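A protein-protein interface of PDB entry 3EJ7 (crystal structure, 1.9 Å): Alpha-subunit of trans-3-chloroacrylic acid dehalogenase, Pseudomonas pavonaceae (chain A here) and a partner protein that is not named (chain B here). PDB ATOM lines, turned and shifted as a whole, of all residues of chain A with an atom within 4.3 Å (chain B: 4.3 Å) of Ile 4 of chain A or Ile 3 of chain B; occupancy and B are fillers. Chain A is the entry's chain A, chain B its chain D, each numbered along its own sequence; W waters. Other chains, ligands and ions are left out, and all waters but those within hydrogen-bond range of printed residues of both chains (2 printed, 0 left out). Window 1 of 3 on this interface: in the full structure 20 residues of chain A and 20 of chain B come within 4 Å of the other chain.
Water W1 bridges the side-chain carboxylate of Glu 4 of chain B (2.7 Å) and the side-chain hydroxyl of Ser 5 of chain A (3.2 Å).
Water W2 lies within hydrogen-bond range of the side-chain hydroxyl (OG) of Ser 5 of chain A (2.7 Å) and the backbone carbonyl oxygen (O) of Phe 2 of chain B (2.9 Å).
Met 3 of chain A touches Glu 4 of chain B (O to O, 3.8 Å).
Met 3 of chain A touches Cys 5 of chain B.
Ile 3 of chain B touches Ile 4 of chain A.
Glu 4 of chain B touches Ile 4 of chain A (O to CA, 3.4 Å).
Phe 2 of chain B touches Ser 5 of chain A.
Ile 3 of chain B touches Ser 5 of chain A.
Phe 2 of chain B touches Cys 6 of chain A.
Printed residues of chain B within 4 Å of Ile 4 of chain A: Ile 3 and Glu 4.
Printed residues of chain A within 4 Å of Ile 3 of chain B: Ile 4 and Ser 5.
Printed residues of chain A within 4 Å of Phe 2 of chain B: Ser 5 (3.6 Å) and Cys 6 (3.3 Å).
Of the printed residues of chain B, Cys 6 of chain A touches Phe 2 (3.3 Å).
Printed residues of chain A within 4 Å of Glu 4 of chain B: Met 3, Ile 4 and Ser 5.
Thr 27 of chain B touches none of the printed residues of chain A.
Val 40 of chain B touches none of the printed residues of chain A.
The nearest printed residue of chain B that does not touch Ile 4 of chain A is Cys 5 of chain B (4.02 Å).
The nearest printed residue of chain B that does not touch Cys 6 of chain A is Pro 1 of chain B (4.1 Å).
Printed residues of chain B that touch a printed residue of chain A: Phe 2, Ile 3, Glu 4 and Cys 5.
Hydrophobic or aromatic side chains of chain B that line the printed part of chain A: Ile 3.
Of the 10 printed residues of chain A, 4 touch a printed residue of chain B.
Printed residues of chain A that touch a printed residue of chain B: Met 3, Ile 4, Ser 5 and Cys 6.
Hydrophobic or aromatic side chains of chain A within 4 Å of the printed part of chain B: Ile 4.
The backbone NH of Ile 4 of chain A is in hydrogen-bond range of the backbone carbonyl oxygen of Phe 40 of chain A (2.8 Å).
The backbone carbonyl oxygen (O) of Ile 4 of chain A is in hydrogen-bond range of the backbone NH (N) of Val 42 of chain A (3.0 Å).
N of Cys 6 of chain A sits at hydrogen-bond distance from O of Val 42 of chain A (2.9 Å).
The backbone carbonyl oxygen of Asn 39 of chain B sits at hydrogen-bond distance from the backbone NH of Ile 3 of chain B.
O of Ile 3 of chain B sits at hydrogen-bond distance from N of Leu 41 of chain B.
The backbone NH (N) of Cys 5 of chain B is in hydrogen-bond range of the backbone carbonyl oxygen (O) of Leu 41 of chain B.
O of Ser 5 of chain A is in hydrogen-bond range of N of Glu 4 of chain B (2.9 Å).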
ATOM      1  N   PRO A   2      29.272  -3.588  11.693  1.00  0.00           N
ATOM      2  CA  PRO A   2      28.965  -2.483  10.806  1.00  0.00           C
ATOM      3  C   PRO A   2      30.236  -1.957  10.174  1.00  0.00           C
ATOM      4  O   PRO A   2      31.343  -2.136  10.726  1.00  0.00           O
ATOM      5  CB  PRO A   2      28.327  -1.461  11.752  1.00  0.00           C
ATOM      6  CG  PRO A   2      27.613  -2.328  12.747  1.00  0.00           C
ATOM      7  CD  PRO A   2      28.570  -3.460  12.981  1.00  0.00           C
ATOM      8  N   MET A   3      30.096  -1.380   8.989  1.00  0.00           N
ATOM      9  CA  MET A   3      31.201  -0.660   8.382  1.00  0.00           C
ATOM     10  C   MET A   3      30.721   0.715   7.994  1.00  0.00           C
ATOM     11  O   MET A   3      29.700   0.860   7.311  1.00  0.00           O
ATOM     12  CB  MET A   3      31.764  -1.384   7.159  1.00  0.00           C
ATOM     13  CG  MET A   3      32.150  -2.813   7.396  1.00  0.00           C
ATOM     14  SD  MET A   3      30.751  -3.938   7.186  1.00  0.00           S
ATOM     15  CE  MET A   3      31.629  -5.499   7.220  1.00  0.00           C
ATOM     16  N   ILE A   4      31.461   1.717   8.430  1.00  0.00           N
ATOM     17  CA  ILE A   4      31.120   3.126   8.152  1.00  0.00           C
ATOM     18  C   ILE A   4      32.253   3.807   7.381  1.00  0.00           C
ATOM     19  O   ILE A   4      33.421   3.631   7.714  1.00  0.00           O
ATOM     20  CB  ILE A   4      30.894   3.892   9.483  1.00  0.00           C
ATOM     21  CG1 ILE A   4      30.107   3.045  10.486  1.00  0.00           C
ATOM     22  CG2 ILE A   4      30.242   5.259   9.224  1.00  0.00           C
ATOM     23  CD1 ILE A   4      30.137   3.562  11.912  1.00  0.00           C
ATOM     24  N   SER A   5      31.897   4.609   6.373  1.00  0.00           N
ATOM     25  CA  SER A   5      32.865   5.450   5.643  1.00  0.00           C
ATOM     26  C   SER A   5      32.391   6.901   5.634  1.00  0.00           C
ATOM     27  O   SER A   5      31.175   7.172   5.626  1.00  0.00           O
ATOM     28  CB  SER A   5      33.059   4.937   4.214  1.00  0.00           C
ATOM     29  OG  SER A   5      31.871   5.075   3.438  1.00  0.00           O
ATOM     30  N   CYS A   6      33.348   7.825   5.632  1.00  0.00           N
ATOM     31  CA  CYS A   6      33.054   9.222   5.482  1.00  0.00           C
ATOM     32  C   CYS A   6      34.012   9.806   4.446  1.00  0.00           C
ATOM     33  O   CYS A   6      35.232   9.827   4.657  1.00  0.00           O
ATOM     34  CB  CYS A   6      33.196   9.929   6.831  1.00  0.00           C
ATOM     35  SG  CYS A   6      33.026  11.773   6.746  1.00  0.00           S
ATOM     36  N   ILE A  28      25.925   4.416  16.029  1.00  0.00           N
ATOM     37  CA  ILE A  28      25.771   3.147  15.311  1.00  0.00           C
ATOM     38  C   ILE A  28      25.705   1.995  16.301  1.00  0.00           C
ATOM     39  O   ILE A  28      24.857   1.114  16.182  1.00  0.00           O
ATOM     40  CB  ILE A  28      26.901   2.904  14.281  1.00  0.00           C
ATOM     41  CG1 ILE A  28      26.703   3.760  13.033  1.00  0.00           C
ATOM     42  CG2 ILE A  28      26.927   1.450  13.808  1.00  0.00           C
ATOM     43  CD1 ILE A  28      27.177   5.171  13.140  1.00  0.00           C
ATOM     44  N   ILE A  39      32.491  -2.178  14.896  1.00  0.00           N
ATOM     45  CA  ILE A  39      32.183  -1.146  13.917  1.00  0.00           C
ATOM     46  C   ILE A  39      33.479  -0.613  13.315  1.00  0.00           C
ATOM     47  O   ILE A  39      34.262   0.023  14.032  1.00  0.00           O
ATOM     48  CB  ILE A  39      31.421   0.024  14.596  1.00  0.00           C
ATOM     49  CG1 ILE A  39      30.070  -0.433  15.148  1.00  0.00           C
ATOM     50  CG2 ILE A  39      31.232   1.167  13.626  1.00  0.00           C
ATOM     51  CD1 ILE A  39      29.573   0.433  16.263  1.00  0.00           C
ATOM     52  N   PHE A  40      33.730  -0.901  12.037  1.00  0.00           N
ATOM     53  CA  PHE A  40      34.867  -0.360  11.306  1.00  0.00           C
ATOM     54  C   PHE A  40      34.569   1.047  10.764  1.00  0.00           C
ATOM     55  O   PHE A  40      33.466   1.295  10.276  1.00  0.00           O
ATOM     56  CB  PHE A  40      35.247  -1.294  10.147  1.00  0.00           C
ATOM     57  CG  PHE A  40      36.263  -0.715   9.204  1.00  0.00           C
ATOM     58  CD1 PHE A  40      37.632  -0.856   9.455  1.00  0.00           C
ATOM     59  CD2 PHE A  40      35.862  -0.016   8.063  1.00  0.00           C
ATOM     60  CE1 PHE A  40      38.575  -0.321   8.572  1.00  0.00           C
ATOM     61  CE2 PHE A  40      36.792   0.525   7.189  1.00  0.00           C
ATOM     62  CZ  PHE A  40      38.160   0.374   7.445  1.00  0.00           C
ATOM     63  N   PHE A  41      35.543   1.956  10.838  1.00  0.00           N
ATOM     64  CA  PHE A  41      35.344   3.300  10.286  1.00  0.00           C
ATOM     65  C   PHE A  41      36.579   3.709   9.444  1.00  0.00           C
ATOM     66  O   PHE A  41      37.737   3.557   9.903  1.00  0.00           O
ATOM     67  CB  PHE A  41      35.089   4.301  11.427  1.00  0.00           C
ATOM     68  CG  PHE A  41      34.793   5.721  10.975  1.00  0.00           C
ATOM     69  CD1 PHE A  41      34.001   5.977   9.849  1.00  0.00           C
ATOM     70  CD2 PHE A  41      35.277   6.805  11.709  1.00  0.00           C
ATOM     71  CE1 PHE A  41      33.721   7.302   9.449  1.00  0.00           C
ATOM     72  CE2 PHE A  41      34.994   8.117  11.342  1.00  0.00           C
ATOM     73  CZ  PHE A  41      34.209   8.371  10.202  1.00  0.00           C
ATOM     74  N   VAL A  42      36.329   4.237   8.247  1.00  0.00           N
ATOM     75  CA  VAL A  42      37.369   4.846   7.401  1.00  0.00           C
ATOM     76  C   VAL A  42      36.942   6.272   6.975  1.00  0.00           C
ATOM     77  O   VAL A  42      35.797   6.484   6.554  1.00  0.00           O
ATOM     78  CB  VAL A  42      37.757   3.980   6.144  1.00  0.00           C
ATOM     79  CG1 VAL A  42      36.579   3.796   5.158  1.00  0.00           C
ATOM     80  CG2 VAL A  42      38.934   4.592   5.377  1.00  0.00           C
ATOM     81  N   PRO B   1      29.976  16.340   3.560  1.00  0.00           N
ATOM     82  CA  PRO B   1      30.523  14.995   3.640  1.00  0.00           C
ATOM     83  C   PRO B   1      29.524  13.940   3.125  1.00  0.00           C
ATOM     84  O   PRO B   1      28.329  14.250   2.932  1.00  0.00           O
ATOM     85  CB  PRO B   1      30.739  14.797   5.140  1.00  0.00           C
ATOM     86  CG  PRO B   1      30.947  16.160   5.686  1.00  0.00           C
ATOM     87  CD  PRO B   1      30.170  17.105   4.811  1.00  0.00           C
ATOM     88  N   PHE B   2      30.002  12.719   2.899  1.00  0.00           N
ATOM     89  CA  PHE B   2      29.101  11.608   2.566  1.00  0.00           C
ATOM     90  C   PHE B   2      29.442  10.467   3.506  1.00  0.00           C
ATOM     91  O   PHE B   2      30.566   9.987   3.480  1.00  0.00           O
ATOM     92  CB  PHE B   2      29.278  11.184   1.112  1.00  0.00           C
ATOM     93  CG  PHE B   2      28.559   9.926   0.737  1.00  0.00           C
ATOM     94  CD1 PHE B   2      27.305   9.646   1.252  1.00  0.00           C
ATOM     95  CD2 PHE B   2      29.102   9.062  -0.220  1.00  0.00           C
ATOM     96  CE1 PHE B   2      26.633   8.501   0.899  1.00  0.00           C
ATOM     97  CE2 PHE B   2      28.414   7.888  -0.602  1.00  0.00           C
ATOM     98  CZ  PHE B   2      27.180   7.610  -0.011  1.00  0.00           C
ATOM     99  N   ILE B   3      28.496  10.104   4.374  1.00  0.00           N
ATOM    100  CA  ILE B   3      28.689   9.021   5.348  1.00  0.00           C
ATOM    101  C   ILE B   3      27.868   7.824   4.828  1.00  0.00           C
ATOM    102  O   ILE B   3      26.630   7.910   4.630  1.00  0.00           O
ATOM    103  CB  ILE B   3      28.269   9.386   6.801  1.00  0.00           C
ATOM    104  CG1 ILE B   3      29.005  10.620   7.348  1.00  0.00           C
ATOM    105  CG2 ILE B   3      28.528   8.199   7.770  1.00  0.00           C
ATOM    106  CD1 ILE B   3      28.269  11.921   7.099  1.00  0.00           C
ATOM    107  N   GLU B   4      28.546   6.719   4.576  1.00  0.00           N
ATOM    108  CA  GLU B   4      27.834   5.517   4.121  1.00  0.00           C
ATOM    109  C   GLU B   4      27.961   4.490   5.250  1.00  0.00           C
ATOM    110  O   GLU B   4      29.078   4.191   5.686  1.00  0.00           O
ATOM    111  CB  GLU B   4      28.407   4.986   2.809  1.00  0.00           C
ATOM    112  CG  GLU B   4      27.773   3.668   2.339  1.00  0.00           C
ATOM    113  CD  GLU B   4      28.188   3.266   0.930  1.00  0.00           C
ATOM    114  OE1 GLU B   4      27.607   2.295   0.387  1.00  0.00           O
ATOM    115  OE2 GLU B   4      29.082   3.904   0.358  1.00  0.00           O
ATOM    116  N   CYS B   5      26.830   3.993   5.738  1.00  0.00           N
ATOM    117  CA  CYS B   5      26.796   3.014   6.856  1.00  0.00           C
ATOM    118  C   CYS B   5      26.252   1.663   6.401  1.00  0.00           C
ATOM    119  O   CYS B   5      25.108   1.542   5.944  1.00  0.00           O
ATOM    120  CB  CYS B   5      25.941   3.514   8.008  1.00  0.00           C
ATOM    121  SG  CYS B   5      26.295   5.164   8.478  1.00  0.00           S
ATOM    122  N   VAL B  23      23.458  10.402  13.087  1.00  0.00           N
ATOM    123  CA  VAL B  23      24.651  10.535  12.204  1.00  0.00           C
ATOM    124  C   VAL B  23      24.844  11.984  11.747  1.00  0.00           C
ATOM    125  O   VAL B  23      25.951  12.500  11.786  1.00  0.00           O
ATOM    126  CB  VAL B  23      24.647   9.577  10.942  1.00  0.00           C
ATOM    127  CG1 VAL B  23      25.714  10.006   9.891  1.00  0.00           C
ATOM    128  CG2 VAL B  23      24.862   8.126  11.344  1.00  0.00           C
ATOM    129  N   THR B  27      27.919  14.514  12.973  1.00  0.00           N
ATOM    130  CA  THR B  27      28.830  14.999  11.948  1.00  0.00           C
ATOM    131  C   THR B  27      28.931  16.502  12.061  1.00  0.00           C
ATOM    132  O   THR B  27      30.026  17.049  12.065  1.00  0.00           O
ATOM    133  CB  THR B  27      28.383  14.534  10.537  1.00  0.00           C
ATOM    134  OG1 THR B  27      28.385  13.099  10.502  1.00  0.00           O
ATOM    135  CG2 THR B  27      29.312  15.066   9.433  1.00  0.00           C
ATOM    136  N   ILE B  38      25.714  17.662   4.443  1.00  0.00           N
ATOM    137  CA  ILE B  38      25.839  16.292   5.039  1.00  0.00           C
ATOM    138  C   ILE B  38      24.915  15.303   4.317  1.00  0.00           C
ATOM    139  O   ILE B  38      23.681  15.491   4.242  1.00  0.00           O
ATOM    140  CB  ILE B  38      25.592  16.261   6.593  1.00  0.00           C
ATOM    141  CG1 ILE B  38      26.590  17.167   7.318  1.00  0.00           C
ATOM    142  CG2 ILE B  38      25.673  14.798   7.127  1.00  0.00           C
ATOM    143  CD1 ILE B  38      26.328  17.362   8.839  1.00  0.00           C
ATOM    144  N   ASN B  39      25.504  14.268   3.743  1.00  0.00           N
ATOM    145  CA  ASN B  39      24.724  13.262   2.999  1.00  0.00           C
ATOM    146  C   ASN B  39      24.954  11.897   3.618  1.00  0.00           C
ATOM    147  O   ASN B  39      26.090  11.550   3.959  1.00  0.00           O
ATOM    148  CB  ASN B  39      25.105  13.280   1.538  1.00  0.00           C
ATOM    149  CG  ASN B  39      24.887  14.659   0.887  1.00  0.00           C
ATOM    150  OD1 ASN B  39      23.799  14.958   0.367  1.00  0.00           O
ATOM    151  ND2 ASN B  39      25.929  15.482   0.894  1.00  0.00           N
ATOM    152  N   VAL B  40      23.869  11.147   3.813  1.00  0.00           N
ATOM    153  CA  VAL B  40      23.935   9.882   4.546  1.00  0.00           C
ATOM    154  C   VAL B  40      23.267   8.758   3.713  1.00  0.00           C
ATOM    155  O   VAL B  40      22.156   8.918   3.145  1.00  0.00           O
ATOM    156  CB  VAL B  40      23.301   9.971   5.950  1.00  0.00           C
ATOM    157  CG1 VAL B  40      23.499   8.628   6.707  1.00  0.00           C
ATOM    158  CG2 VAL B  40      23.894  11.103   6.783  1.00  0.00           C
ATOM    159  N   LEU B  41      23.966   7.641   3.621  1.00  0.00           N
ATOM    160  CA  LEU B  41      23.414   6.452   2.989  1.00  0.00           C
ATOM    161  C   LEU B  41      23.480   5.269   3.956  1.00  0.00           C
ATOM    162  O   LEU B  41      24.576   4.869   4.408  1.00  0.00           O
ATOM    163  CB  LEU B  41      24.191   6.138   1.728  1.00  0.00           C
ATOM    164  CG  LEU B  41      23.589   5.390   0.523  1.00  0.00           C
ATOM    165  CD1 LEU B  41      24.519   4.304   0.004  1.00  0.00           C
ATOM    166  CD2 LEU B  41      22.153   4.883   0.730  1.00  0.00           C
HETATM  167  O   HOH W   1      31.051   5.759   0.432  1.00  0.00           O
HETATM  168  O   HOH W   2      31.598   7.540   2.299  1.00  0.00           O
